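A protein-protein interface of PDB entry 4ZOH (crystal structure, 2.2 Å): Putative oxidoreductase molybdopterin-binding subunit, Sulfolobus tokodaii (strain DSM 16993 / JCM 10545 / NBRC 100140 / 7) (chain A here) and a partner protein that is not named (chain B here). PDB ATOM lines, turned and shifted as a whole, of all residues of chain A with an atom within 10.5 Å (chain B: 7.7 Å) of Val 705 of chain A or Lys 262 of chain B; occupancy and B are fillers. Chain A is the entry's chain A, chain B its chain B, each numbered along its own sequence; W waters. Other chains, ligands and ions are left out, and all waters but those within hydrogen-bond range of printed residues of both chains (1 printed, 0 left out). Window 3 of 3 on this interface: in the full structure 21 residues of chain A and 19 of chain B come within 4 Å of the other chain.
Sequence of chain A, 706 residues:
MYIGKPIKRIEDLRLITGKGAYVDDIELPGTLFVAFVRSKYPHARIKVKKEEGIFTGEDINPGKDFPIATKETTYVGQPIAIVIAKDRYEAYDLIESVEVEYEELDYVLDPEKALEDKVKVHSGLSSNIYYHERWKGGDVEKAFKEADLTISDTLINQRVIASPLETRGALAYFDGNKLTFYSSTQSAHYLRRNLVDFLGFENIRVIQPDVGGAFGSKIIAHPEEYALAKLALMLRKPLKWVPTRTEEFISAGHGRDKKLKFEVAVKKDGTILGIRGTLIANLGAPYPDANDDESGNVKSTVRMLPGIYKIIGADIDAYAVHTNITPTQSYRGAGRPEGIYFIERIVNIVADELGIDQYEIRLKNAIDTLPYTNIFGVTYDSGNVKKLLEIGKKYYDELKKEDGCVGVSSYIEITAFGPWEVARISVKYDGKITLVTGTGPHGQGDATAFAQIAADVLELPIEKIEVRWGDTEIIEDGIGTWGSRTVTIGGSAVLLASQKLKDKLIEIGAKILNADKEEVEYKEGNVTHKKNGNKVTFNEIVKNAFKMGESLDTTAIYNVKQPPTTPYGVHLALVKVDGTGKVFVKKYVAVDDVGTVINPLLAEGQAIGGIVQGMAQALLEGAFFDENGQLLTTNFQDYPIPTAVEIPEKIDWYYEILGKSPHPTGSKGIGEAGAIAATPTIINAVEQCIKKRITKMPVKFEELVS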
ATOM      1  N   VAL A 577       0.570   2.194 -13.325  1.00  0.00           N
ATOM      2  CA  VAL A 577       1.262   0.914 -13.384  1.00  0.00           C
ATOM      3  C   VAL A 577       0.163  -0.084 -13.188  1.00  0.00           C
ATOM      4  O   VAL A 577      -0.709   0.183 -12.400  1.00  0.00           O
ATOM      5  CB  VAL A 577       2.315   0.783 -12.242  1.00  0.00           C
ATOM      6  CG1 VAL A 577       3.040  -0.536 -12.289  1.00  0.00           C
ATOM      7  CG2 VAL A 577       3.335   1.900 -12.356  1.00  0.00           C
ATOM      8  N   ASP A 578       0.175  -1.211 -13.892  1.00  0.00           N
ATOM      9  CA  ASP A 578      -0.920  -2.169 -13.788  1.00  0.00           C
ATOM     10  C   ASP A 578      -0.449  -3.339 -13.006  1.00  0.00           C
ATOM     11  O   ASP A 578       0.667  -3.324 -12.477  1.00  0.00           O
ATOM     12  CB  ASP A 578      -1.572  -2.536 -15.147  1.00  0.00           C
ATOM     13  CG  ASP A 578      -0.721  -3.423 -16.020  1.00  0.00           C
ATOM     14  OD1 ASP A 578      -1.028  -3.482 -17.218  1.00  0.00           O
ATOM     15  OD2 ASP A 578       0.258  -4.066 -15.570  1.00  0.00           O
ATOM     16  N   GLY A 579      -1.287  -4.369 -12.904  1.00  0.00           N
ATOM     17  CA  GLY A 579      -0.918  -5.554 -12.120  1.00  0.00           C
ATOM     18  C   GLY A 579       0.153  -6.437 -12.705  1.00  0.00           C
ATOM     19  O   GLY A 579       0.510  -7.436 -12.085  1.00  0.00           O
ATOM     20  N   THR A 580       0.652  -6.111 -13.906  1.00  0.00           N
ATOM     21  CA  THR A 580       1.775  -6.875 -14.528  1.00  0.00           C
ATOM     22  C   THR A 580       3.085  -6.108 -14.334  1.00  0.00           C
ATOM     23  O   THR A 580       4.184  -6.594 -14.646  1.00  0.00           O
ATOM     24  CB  THR A 580       1.559  -7.159 -16.041  1.00  0.00           C
ATOM     25  OG1 THR A 580       1.502  -5.928 -16.761  1.00  0.00           O
ATOM     26  CG2 THR A 580       0.245  -7.988 -16.296  1.00  0.00           C
ATOM     27  N   GLY A 581       2.962  -4.914 -13.777  1.00  0.00           N
ATOM     28  CA  GLY A 581       4.099  -4.049 -13.611  1.00  0.00           C
ATOM     29  C   GLY A 581       4.457  -3.211 -14.830  1.00  0.00           C
ATOM     30  O   GLY A 581       5.512  -2.547 -14.826  1.00  0.00           O
ATOM     31  N   LYS A 582       3.550  -3.170 -15.812  1.00  0.00           N
ATOM     32  CA  LYS A 582       3.712  -2.337 -16.988  1.00  0.00           C
ATOM     33  C   LYS A 582       3.304  -0.907 -16.704  1.00  0.00           C
ATOM     34  O   LYS A 582       2.261  -0.654 -16.099  1.00  0.00           O
ATOM     35  CB  LYS A 582       2.911  -2.912 -18.178  1.00  0.00           C
ATOM     36  CG  LYS A 582       3.077  -2.075 -19.453  1.00  0.00           C
ATOM     37  CD  LYS A 582       2.234  -2.551 -20.617  1.00  0.00           C
ATOM     38  CE  LYS A 582       2.815  -3.781 -21.243  1.00  0.00           C
ATOM     39  NZ  LYS A 582       2.797  -3.614 -22.712  1.00  0.00           N
ATOM     40  N   VAL A 583       4.121   0.021 -17.159  1.00  0.00           N
ATOM     41  CA  VAL A 583       3.917   1.417 -16.980  1.00  0.00           C
ATOM     42  C   VAL A 583       3.224   2.020 -18.190  1.00  0.00           C
ATOM     43  O   VAL A 583       3.669   1.809 -19.281  1.00  0.00           O
ATOM     44  CB  VAL A 583       5.276   2.107 -16.768  1.00  0.00           C
ATOM     45  CG1 VAL A 583       5.155   3.638 -16.699  1.00  0.00           C
ATOM     46  CG2 VAL A 583       5.907   1.636 -15.455  1.00  0.00           C
ATOM     47  N   VAL A 686       6.975   7.247 -11.765  1.00  0.00           N
ATOM     48  CA  VAL A 686       6.765   5.841 -11.433  1.00  0.00           C
ATOM     49  C   VAL A 686       7.001   5.624  -9.935  1.00  0.00           C
ATOM     50  O   VAL A 686       6.394   4.734  -9.298  1.00  0.00           O
ATOM     51  CB  VAL A 686       7.679   4.903 -12.215  1.00  0.00           C
ATOM     52  CG1 VAL A 686       7.471   3.428 -11.820  1.00  0.00           C
ATOM     53  CG2 VAL A 686       7.394   4.991 -13.710  1.00  0.00           C
ATOM     54  N   CYS A 689       4.087   6.236  -7.818  1.00  0.00           N
ATOM     55  CA  CYS A 689       3.182   5.055  -7.823  1.00  0.00           C
ATOM     56  C   CYS A 689       3.643   3.822  -7.046  1.00  0.00           C
ATOM     57  O   CYS A 689       2.870   2.911  -6.898  1.00  0.00           O
ATOM     58  CB  CYS A 689       2.678   4.667  -9.283  1.00  0.00           C
ATOM     59  SG  CYS A 689       1.054   5.391  -9.790  1.00  0.00           S
ATOM     60  N   ILE A 690       4.872   3.698  -6.565  1.00  0.00           N
ATOM     61  CA  ILE A 690       5.211   2.307  -6.161  1.00  0.00           C
ATOM     62  C   ILE A 690       5.228   1.740  -4.758  1.00  0.00           C
ATOM     63  O   ILE A 690       4.856   0.573  -4.606  1.00  0.00           O
ATOM     64  CB  ILE A 690       6.378   1.605  -6.894  1.00  0.00           C
ATOM     65  CG1 ILE A 690       7.547   2.561  -7.151  1.00  0.00           C
ATOM     66  CG2 ILE A 690       5.833   0.770  -8.042  1.00  0.00           C
ATOM     67  CD1 ILE A 690       8.832   1.820  -7.467  1.00  0.00           C
ATOM     68  N   LYS A 691       5.700   2.412  -3.728  1.00  0.00           N
ATOM     69  CA  LYS A 691       6.461   3.599  -3.726  1.00  0.00           C
ATOM     70  C   LYS A 691       7.621   2.980  -2.913  1.00  0.00           C
ATOM     71  O   LYS A 691       7.517   2.780  -1.703  1.00  0.00           O
ATOM     72  CB  LYS A 691       5.701   4.707  -2.977  1.00  0.00           C
ATOM     73  CG  LYS A 691       4.297   4.319  -2.488  1.00  0.00           C
ATOM     74  CD  LYS A 691       3.520   5.500  -1.934  1.00  0.00           C
ATOM     75  CE  LYS A 691       2.375   5.891  -2.858  1.00  0.00           C
ATOM     76  NZ  LYS A 691       2.165   7.376  -2.864  1.00  0.00           N
ATOM     77  N   LYS A 692       8.630   2.493  -3.646  1.00  0.00           N
ATOM     78  CA  LYS A 692       9.951   2.208  -3.130  1.00  0.00           C
ATOM     79  C   LYS A 692      10.862   3.132  -3.900  1.00  0.00           C
ATOM     80  O   LYS A 692      10.483   3.698  -4.935  1.00  0.00           O
ATOM     81  CB  LYS A 692      10.430   0.785  -3.415  1.00  0.00           C
ATOM     82  CG  LYS A 692       9.395  -0.303  -3.605  1.00  0.00           C
ATOM     83  CD  LYS A 692      10.142  -1.594  -3.961  1.00  0.00           C
ATOM     84  CE  LYS A 692      10.275  -1.786  -5.473  1.00  0.00           C
ATOM     85  NZ  LYS A 692      10.576  -3.178  -5.948  1.00  0.00           N
ATOM     86  N   VAL A 699      13.171   0.481 -15.525  1.00  0.00           N
ATOM     87  CA  VAL A 699      12.356  -0.119 -14.478  1.00  0.00           C
ATOM     88  C   VAL A 699      11.820  -1.427 -15.032  1.00  0.00           C
ATOM     89  O   VAL A 699      11.087  -1.456 -16.009  1.00  0.00           O
ATOM     90  CB  VAL A 699      11.227   0.842 -14.045  1.00  0.00           C
ATOM     91  CG1 VAL A 699      10.752   0.504 -12.662  1.00  0.00           C
ATOM     92  CG2 VAL A 699      11.752   2.246 -13.915  1.00  0.00           C
ATOM     93  N   LYS A 700      12.181  -2.537 -14.444  1.00  0.00           N
ATOM     94  CA  LYS A 700      11.620  -3.791 -14.952  1.00  0.00           C
ATOM     95  C   LYS A 700      10.177  -4.066 -14.443  1.00  0.00           C
ATOM     96  O   LYS A 700       9.835  -3.701 -13.308  1.00  0.00           O
ATOM     97  CB  LYS A 700      12.509  -4.966 -14.540  1.00  0.00           C
ATOM     98  CG  LYS A 700      13.916  -5.036 -15.198  1.00  0.00           C
ATOM     99  CD  LYS A 700      14.656  -6.240 -14.576  1.00  0.00           C
ATOM    100  CE  LYS A 700      15.479  -7.061 -15.551  1.00  0.00           C
ATOM    101  NZ  LYS A 700      16.892  -6.949 -15.115  1.00  0.00           N
ATOM    102  N   PHE A 701       9.359  -4.751 -15.252  1.00  0.00           N
ATOM    103  CA  PHE A 701       8.025  -5.217 -14.838  1.00  0.00           C
ATOM    104  C   PHE A 701       8.053  -5.870 -13.429  1.00  0.00           C
ATOM    105  O   PHE A 701       7.285  -5.454 -12.534  1.00  0.00           O
ATOM    106  CB  PHE A 701       7.435  -6.204 -15.891  1.00  0.00           C
ATOM    107  CG  PHE A 701       7.034  -5.562 -17.203  1.00  0.00           C
ATOM    108  CD1 PHE A 701       7.297  -4.195 -17.477  1.00  0.00           C
ATOM    109  CD2 PHE A 701       6.411  -6.321 -18.190  1.00  0.00           C
ATOM    110  CE1 PHE A 701       6.945  -3.616 -18.688  1.00  0.00           C
ATOM    111  CE2 PHE A 701       6.033  -5.737 -19.418  1.00  0.00           C
ATOM    112  CZ  PHE A 701       6.297  -4.383 -19.658  1.00  0.00           C
ATOM    113  N   GLU A 702       8.949  -6.846 -13.231  1.00  0.00           N
ATOM    114  CA  GLU A 702       9.030  -7.597 -11.947  1.00  0.00           C
ATOM    115  C   GLU A 702       9.409  -6.758 -10.737  1.00  0.00           C
ATOM    116  O   GLU A 702       9.177  -7.188  -9.630  1.00  0.00           O
ATOM    117  CB  GLU A 702       9.986  -8.758 -12.027  1.00  0.00           C
ATOM    118  CG  GLU A 702      11.397  -8.404 -12.462  1.00  0.00           C
ATOM    119  CD  GLU A 702      12.133  -9.607 -13.039  1.00  0.00           C
ATOM    120  OE1 GLU A 702      11.631 -10.311 -13.968  1.00  0.00           O
ATOM    121  OE2 GLU A 702      13.253  -9.852 -12.555  1.00  0.00           O
ATOM    122  N   GLU A 703       9.992  -5.583 -10.962  1.00  0.00           N
ATOM    123  CA  GLU A 703      10.342  -4.669  -9.886  1.00  0.00           C
ATOM    124  C   GLU A 703       9.132  -3.851  -9.447  1.00  0.00           C
ATOM    125  O   GLU A 703       9.216  -3.128  -8.472  1.00  0.00           O
ATOM    126  CB  GLU A 703      11.489  -3.735 -10.325  1.00  0.00           C
ATOM    127  CG  GLU A 703      12.885  -4.359 -10.271  1.00  0.00           C
ATOM    128  CD  GLU A 703      13.939  -3.681 -11.170  1.00  0.00           C
ATOM    129  OE1 GLU A 703      13.713  -2.586 -11.781  1.00  0.00           O
ATOM    130  OE2 GLU A 703      15.034  -4.283 -11.283  1.00  0.00           O
ATOM    131  N   LEU A 704       8.028  -3.936 -10.196  1.00  0.00           N
ATOM    132  CA  LEU A 704       6.854  -3.126  -9.937  1.00  0.00           C
ATOM    133  C   LEU A 704       5.585  -3.965  -9.579  1.00  0.00           C
ATOM    134  O   LEU A 704       4.465  -3.529  -9.767  1.00  0.00           O
ATOM    135  CB  LEU A 704       6.586  -2.227 -11.146  1.00  0.00           C
ATOM    136  CG  LEU A 704       7.627  -1.232 -11.614  1.00  0.00           C
ATOM    137  CD1 LEU A 704       7.026  -0.300 -12.652  1.00  0.00           C
ATOM    138  CD2 LEU A 704       8.154  -0.428 -10.444  1.00  0.00           C
ATOM    139  N   VAL A 705       5.764  -5.170  -9.064  1.00  0.00           N
ATOM    140  CA  VAL A 705       4.637  -6.035  -8.845  1.00  0.00           C
ATOM    141  C   VAL A 705       4.583  -6.422  -7.369  1.00  0.00           C
ATOM    142  O   VAL A 705       5.584  -6.850  -6.830  1.00  0.00           O
ATOM    143  CB  VAL A 705       4.687  -7.183  -9.891  1.00  0.00           C
ATOM    144  CG1 VAL A 705       4.430  -8.576  -9.324  1.00  0.00           C
ATOM    145  CG2 VAL A 705       3.738  -6.856 -11.026  1.00  0.00           C
ATOM    146  N   LEU B 179       0.835 -11.152 -22.417  1.00  0.00           N
ATOM    147  CA  LEU B 179       1.718 -10.183 -21.758  1.00  0.00           C
ATOM    148  C   LEU B 179       2.929  -9.931 -22.665  1.00  0.00           C
ATOM    149  O   LEU B 179       3.594 -10.911 -23.145  1.00  0.00           O
ATOM    150  CB  LEU B 179       2.157 -10.680 -20.360  1.00  0.00           C
ATOM    151  CG  LEU B 179       3.194  -9.856 -19.575  1.00  0.00           C
ATOM    152  CD1 LEU B 179       2.766  -8.443 -19.271  1.00  0.00           C
ATOM    153  CD2 LEU B 179       3.536 -10.594 -18.289  1.00  0.00           C
ATOM    154  N   VAL B 189       4.125 -13.995 -21.303  1.00  0.00           N
ATOM    155  CA  VAL B 189       3.181 -15.015 -20.832  1.00  0.00           C
ATOM    156  C   VAL B 189       1.922 -14.940 -21.732  1.00  0.00           C
ATOM    157  O   VAL B 189       1.455 -13.854 -22.042  1.00  0.00           O
ATOM    158  CB  VAL B 189       2.791 -14.779 -19.350  1.00  0.00           C
ATOM    159  CG1 VAL B 189       1.758 -15.826 -18.960  1.00  0.00           C
ATOM    160  CG2 VAL B 189       4.024 -14.850 -18.409  1.00  0.00           C
ATOM    161  N   ALA B 240      -7.161 -18.747 -10.489  1.00  0.00           N
ATOM    162  CA  ALA B 240      -6.046 -17.930 -10.999  1.00  0.00           C
ATOM    163  C   ALA B 240      -4.746 -18.360 -10.277  1.00  0.00           C
ATOM    164  O   ALA B 240      -3.705 -18.588 -10.926  1.00  0.00           O
ATOM    165  CB  ALA B 240      -6.323 -16.418 -10.858  1.00  0.00           C
ATOM    166  N   MET B 244      -0.844 -21.270 -11.756  1.00  0.00           N
ATOM    167  CA  MET B 244       0.611 -21.290 -11.461  1.00  0.00           C
ATOM    168  C   MET B 244       1.194 -22.680 -11.316  1.00  0.00           C
ATOM    169  O   MET B 244       2.388 -22.863 -11.575  1.00  0.00           O
ATOM    170  CB  MET B 244       0.937 -20.459 -10.224  1.00  0.00           C
ATOM    171  CG  MET B 244       0.501 -19.036 -10.369  1.00  0.00           C
ATOM    172  SD  MET B 244       1.361 -17.898  -9.314  1.00  0.00           S
ATOM    173  CE  MET B 244       0.722 -18.503  -7.743  1.00  0.00           C
ATOM    174  N   ALA B 247       2.725 -23.905 -14.610  1.00  0.00           N
ATOM    175  CA  ALA B 247       3.787 -23.060 -15.229  1.00  0.00           C
ATOM    176  C   ALA B 247       5.163 -23.484 -14.763  1.00  0.00           C
ATOM    177  O   ALA B 247       5.432 -23.446 -13.571  1.00  0.00           O
ATOM    178  CB  ALA B 247       3.569 -21.571 -14.941  1.00  0.00           C
ATOM    179  N   PRO B 249       8.268 -21.869 -15.949  1.00  0.00           N
ATOM    180  CA  PRO B 249       8.966 -20.903 -16.818  1.00  0.00           C
ATOM    181  C   PRO B 249      10.494 -20.752 -16.592  1.00  0.00           C
ATOM    182  O   PRO B 249      11.016 -21.340 -15.673  1.00  0.00           O
ATOM    183  CB  PRO B 249       8.252 -19.594 -16.510  1.00  0.00           C
ATOM    184  CG  PRO B 249       7.884 -19.729 -15.073  1.00  0.00           C
ATOM    185  CD  PRO B 249       7.543 -21.168 -14.865  1.00  0.00           C
ATOM    186  N   SER B 256      12.164 -12.652 -15.081  1.00  0.00           N
ATOM    187  CA  SER B 256      12.393 -13.768 -14.114  1.00  0.00           C
ATOM    188  C   SER B 256      11.430 -14.975 -14.261  1.00  0.00           C
ATOM    189  O   SER B 256      10.248 -14.792 -14.610  1.00  0.00           O
ATOM    190  CB  SER B 256      12.147 -13.155 -12.757  1.00  0.00           C
ATOM    191  OG  SER B 256      12.725 -13.944 -11.766  1.00  0.00           O
ATOM    192  N   ALA B 257      11.877 -16.198 -13.974  1.00  0.00           N
ATOM    193  CA  ALA B 257      10.957 -17.345 -13.855  1.00  0.00           C
ATOM    194  C   ALA B 257       9.891 -17.115 -12.783  1.00  0.00           C
ATOM    195  O   ALA B 257       8.726 -17.484 -12.959  1.00  0.00           O
ATOM    196  CB  ALA B 257      11.705 -18.648 -13.569  1.00  0.00           C
ATOM    197  N   GLU B 258      10.274 -16.455 -11.700  1.00  0.00           N
ATOM    198  CA  GLU B 258       9.346 -16.178 -10.629  1.00  0.00           C
ATOM    199  C   GLU B 258       8.275 -15.139 -11.001  1.00  0.00           C
ATOM    200  O   GLU B 258       7.113 -15.253 -10.591  1.00  0.00           O
ATOM    201  CB  GLU B 258      10.095 -15.710  -9.378  1.00  0.00           C
ATOM    202  CG  GLU B 258       9.193 -15.574  -8.156  1.00  0.00           C
ATOM    203  CD  GLU B 258       9.920 -15.065  -6.924  1.00  0.00           C
ATOM    204  OE1 GLU B 258      11.120 -14.677  -7.034  1.00  0.00           O
ATOM    205  OE2 GLU B 258       9.278 -15.054  -5.841  1.00  0.00           O
ATOM    206  N   TYR B 259       8.700 -14.098 -11.711  1.00  0.00           N
ATOM    207  CA  TYR B 259       7.798 -13.070 -12.169  1.00  0.00           C
ATOM    208  C   TYR B 259       6.761 -13.646 -13.143  1.00  0.00           C
ATOM    209  O   TYR B 259       5.581 -13.313 -13.038  1.00  0.00           O
ATOM    210  CB  TYR B 259       8.549 -11.898 -12.790  1.00  0.00           C
ATOM    211  CG  TYR B 259       7.670 -11.028 -13.656  1.00  0.00           C
ATOM    212  CD1 TYR B 259       6.859 -10.004 -13.076  1.00  0.00           C
ATOM    213  CD2 TYR B 259       7.629 -11.216 -15.067  1.00  0.00           C
ATOM    214  CE1 TYR B 259       6.078  -9.170 -13.878  1.00  0.00           C
ATOM    215  CE2 TYR B 259       6.835 -10.398 -15.882  1.00  0.00           C
ATOM    216  CZ  TYR B 259       6.058  -9.393 -15.293  1.00  0.00           C
ATOM    217  OH  TYR B 259       5.274  -8.609 -16.056  1.00  0.00           O
ATOM    218  N   LYS B 260       7.223 -14.530 -14.024  1.00  0.00           N
ATOM    219  CA  LYS B 260       6.416 -15.139 -15.042  1.00  0.00           C
ATOM    220  C   LYS B 260       5.327 -16.019 -14.424  1.00  0.00           C
ATOM    221  O   LYS B 260       4.185 -15.994 -14.885  1.00  0.00           O
ATOM    222  CB  LYS B 260       7.292 -15.966 -15.984  1.00  0.00           C
ATOM    223  CG  LYS B 260       8.023 -15.140 -17.048  1.00  0.00           C
ATOM    224  CD  LYS B 260       9.046 -16.009 -17.721  1.00  0.00           C
ATOM    225  CE  LYS B 260       9.953 -15.227 -18.650  1.00  0.00           C
ATOM    226  NZ  LYS B 260      10.447 -16.256 -19.612  1.00  0.00           N
ATOM    227  N   LYS B 261       5.710 -16.825 -13.426  1.00  0.00           N
ATOM    228  CA  LYS B 261       4.797 -17.710 -12.699  1.00  0.00           C
ATOM    229  C   LYS B 261       3.694 -16.847 -12.056  1.00  0.00           C
ATOM    230  O   LYS B 261       2.533 -17.112 -12.256  1.00  0.00           O
ATOM    231  CB  LYS B 261       5.577 -18.493 -11.651  1.00  0.00           C
ATOM    232  CG  LYS B 261       4.885 -19.742 -11.184  1.00  0.00           C
ATOM    233  CD  LYS B 261       5.544 -20.244  -9.910  1.00  0.00           C
ATOM    234  CE  LYS B 261       4.900 -21.542  -9.407  1.00  0.00           C
ATOM    235  NZ  LYS B 261       5.286 -22.736 -10.210  1.00  0.00           N
ATOM    236  N   LYS B 262       4.080 -15.778 -11.359  1.00  0.00           N
ATOM    237  CA  LYS B 262       3.151 -14.797 -10.815  1.00  0.00           C
ATOM    238  C   LYS B 262       2.258 -14.205 -11.884  1.00  0.00           C
ATOM    239  O   LYS B 262       1.032 -14.114 -11.682  1.00  0.00           O
ATOM    240  CB  LYS B 262       3.862 -13.697 -10.012  1.00  0.00           C
ATOM    241  CG  LYS B 262       4.535 -14.188  -8.714  1.00  0.00           C
ATOM    242  CD  LYS B 262       5.420 -13.141  -8.030  1.00  0.00           C
ATOM    243  CE  LYS B 262       4.588 -11.965  -7.497  1.00  0.00           C
ATOM    244  NZ  LYS B 262       5.391 -10.780  -7.059  1.00  0.00           N
ATOM    245  N   MET B 263       2.832 -13.877 -13.048  1.00  0.00           N
ATOM    246  CA  MET B 263       2.002 -13.375 -14.148  1.00  0.00           C
ATOM    247  C   MET B 263       0.994 -14.376 -14.674  1.00  0.00           C
ATOM    248  O   MET B 263      -0.034 -13.951 -15.208  1.00  0.00           O
ATOM    249  CB  MET B 263       2.832 -12.751 -15.284  1.00  0.00           C
ATOM    250  CG  MET B 263       3.574 -11.546 -14.749  1.00  0.00           C
ATOM    251  SD  MET B 263       2.577 -10.220 -14.085  1.00  0.00           S
ATOM    252  CE  MET B 263       2.743 -10.331 -12.272  1.00  0.00           C
ATOM    253  N   VAL B 264       1.237 -15.683 -14.509  1.00  0.00           N
ATOM    254  CA  VAL B 264       0.226 -16.652 -14.936  1.00  0.00           C
ATOM    255  C   VAL B 264      -1.095 -16.397 -14.160  1.00  0.00           C
ATOM    256  O   VAL B 264      -2.212 -16.373 -14.749  1.00  0.00           O
ATOM    257  CB  VAL B 264       0.721 -18.086 -14.824  1.00  0.00           C
ATOM    258  CG1 VAL B 264      -0.417 -19.097 -14.915  1.00  0.00           C
ATOM    259  CG2 VAL B 264       1.728 -18.343 -15.923  1.00  0.00           C
ATOM    260  N   LYS B 265      -0.952 -16.129 -12.859  1.00  0.00           N
ATOM    261  CA  LYS B 265      -2.117 -15.861 -12.039  1.00  0.00           C
ATOM    262  C   LYS B 265      -2.811 -14.577 -12.484  1.00  0.00           C
ATOM    263  O   LYS B 265      -4.023 -14.559 -12.620  1.00  0.00           O
ATOM    264  CB  LYS B 265      -1.765 -15.803 -10.542  1.00  0.00           C
ATOM    265  CG  LYS B 265      -2.821 -15.093  -9.695  1.00  0.00           C
ATOM    266  CD  LYS B 265      -2.217 -14.583  -8.393  1.00  0.00           C
ATOM    267  CE  LYS B 265      -2.640 -15.471  -7.263  1.00  0.00           C
ATOM    268  NZ  LYS B 265      -3.935 -14.901  -6.827  1.00  0.00           N
ATOM    269  N   VAL B 266      -2.039 -13.516 -12.712  1.00  0.00           N
ATOM    270  CA  VAL B 266      -2.601 -12.252 -13.116  1.00  0.00           C
ATOM    271  C   VAL B 266      -3.406 -12.399 -14.448  1.00  0.00           C
ATOM    272  O   VAL B 266      -4.544 -11.907 -14.537  1.00  0.00           O
ATOM    273  CB  VAL B 266      -1.518 -11.139 -13.130  1.00  0.00           C
ATOM    274  CG1 VAL B 266      -2.110  -9.871 -13.686  1.00  0.00           C
ATOM    275  CG2 VAL B 266      -0.951 -10.902 -11.692  1.00  0.00           C
ATOM    276  N   LEU B 267      -2.840 -13.130 -15.425  1.00  0.00           N
ATOM    277  CA  LEU B 267      -3.430 -13.238 -16.763  1.00  0.00           C
ATOM    278  C   LEU B 267      -4.618 -14.201 -16.825  1.00  0.00           C
ATOM    279  O   LEU B 267      -5.551 -13.919 -17.547  1.00  0.00           O
ATOM    280  CB  LEU B 267      -2.418 -13.541 -17.894  1.00  0.00           C
ATOM    281  CG  LEU B 267      -1.243 -12.633 -18.378  1.00  0.00           C
ATOM    282  CD1 LEU B 267      -0.887 -12.775 -19.877  1.00  0.00           C
ATOM    283  CD2 LEU B 267      -1.318 -11.181 -17.966  1.00  0.00           C
ATOM    284  N   THR B 268      -4.548 -15.323 -16.097  1.00  0.00           N
ATOM    285  CA  THR B 268      -5.722 -16.186 -15.853  1.00  0.00           C
ATOM    286  C   THR B 268      -6.871 -15.363 -15.240  1.00  0.00           C
ATOM    287  O   THR B 268      -7.973 -15.371 -15.755  1.00  0.00           O
ATOM    288  CB  THR B 268      -5.358 -17.352 -14.970  1.00  0.00           C
ATOM    289  OG1 THR B 268      -4.285 -18.049 -15.597  1.00  0.00           O
ATOM    290  CG2 THR B 268      -6.479 -18.329 -14.822  1.00  0.00           C
HETATM  291  O   HOH W   1       7.937  -9.588  -9.108  1.00  0.00           O
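The side-chain hydroxyl (OH) of Tyr 259 of chain B lies within hydrogen-bond range of the backbone carbonyl oxygen (O) of Thr 580 of chain A.
The side-chain carboxylate of Glu 702 of chain A sits at hydrogen-bond distance from the backbone NH of Ser 256 of chain B (2.6 Å).
The side-chain hydroxyl (OH) of Tyr 259 of chain B sits close to the side-chain sulfur (SD) of Met 263 of chain B, at 3.7 Å.
O of Val 189 of chain B lies within hydrogen-bond range of N of Leu 179 of chain B, at 2.8 Å.
The side-chain carboxylate (OD2) of Asp 578 of chain A sits at hydrogen-bond distance from the side-chain hydroxyl (OG1) of Thr 580 of chain A (2.5 Å).
Met 263 of chain B touches Gly 579 of chain A.
Gly 579 of chain A touches Val 266 of chain B (O to CG2, 3.8 Å).
CB of Thr 580 of chain A touches CD1 of Leu 179 of chain B, 3.7 Å away.
Met 263 of chain B touches Thr 580 of chain A (SD to CA, 3.5 Å).
Val 266 of chain B touches Thr 580 of chain A.
Thr 580 of chain A touches Leu 267 of chain B (CG2 to CD2, 3.9 Å).
Phe 701 of chain A touches Tyr 259 of chain B.
Glu 702 of chain A touches Tyr 259 of chain B (CA to CD1, 3.4 Å).
Val 705 of chain A touches Lys 262 of chain B (CG1 to NZ, 3.3 Å).
CE of Met 263 of chain B touches CG1 of Val 705 of chain A, at 3.8 Å.
Lys 700 of chain A touches none of the printed residues of chain B.
Val 705 of chain A touches just these residues of chain B: Lys 262 (3.3 Å) and Met 263 (3.8 Å).
Printed residues of chain A within 4 Å of Leu 179 of chain B: Thr 580.
Met 244 of chain B touches none of the printed residues of chain A.
Of the printed residues of chain A, Ser 256 of chain B touches Glu 702.
Of the printed residues of chain A, Tyr 259 of chain B touches Thr 580, Phe 701 and Glu 702.
Of the printed residues of chain A, Lys 262 of chain B touches Val 705.
Of the printed residues of chain A, Val 266 of chain B touches Gly 579 (3.8 Å) and Thr 580 (3.99 Å).
The nearest residue of chain A that does not touch Lys 262 of chain B is Glu 702 of chain A (5.8 Å).
Of the 19 printed residues of chain A, 5 touch a printed residue of chain B.
Hydrophobic or aromatic side chains of chain A within 4 Å of the printed part of chain B: Phe 701 and Val 705.
Of the 19 printed residues of chain B, 7 touch a printed residue of chain A.
Printed residues of chain B that touch a printed residue of chain A: Leu 179, Ser 256, Tyr 259, Lys 262, Met 263, Val 266 and Leu 267.
Hydrophobic or aromatic side chains of chain B within 4 Å of the printed part of chain A: Leu 179, Tyr 259, Met 263, Val 266 and Leu 267.
Along chain B the printed residues that touch a printed residue of chain A span positions 179 to 267.
Among the printed residues, no Asp or Glu carboxylate lies within 4 Å of a Lys or Arg side-chain nitrogen of the other chain.
Water W1 bridges O of Glu 702 of chain A (2.8 Å) and NZ of Lys 262 of chain B (3.5 Å).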
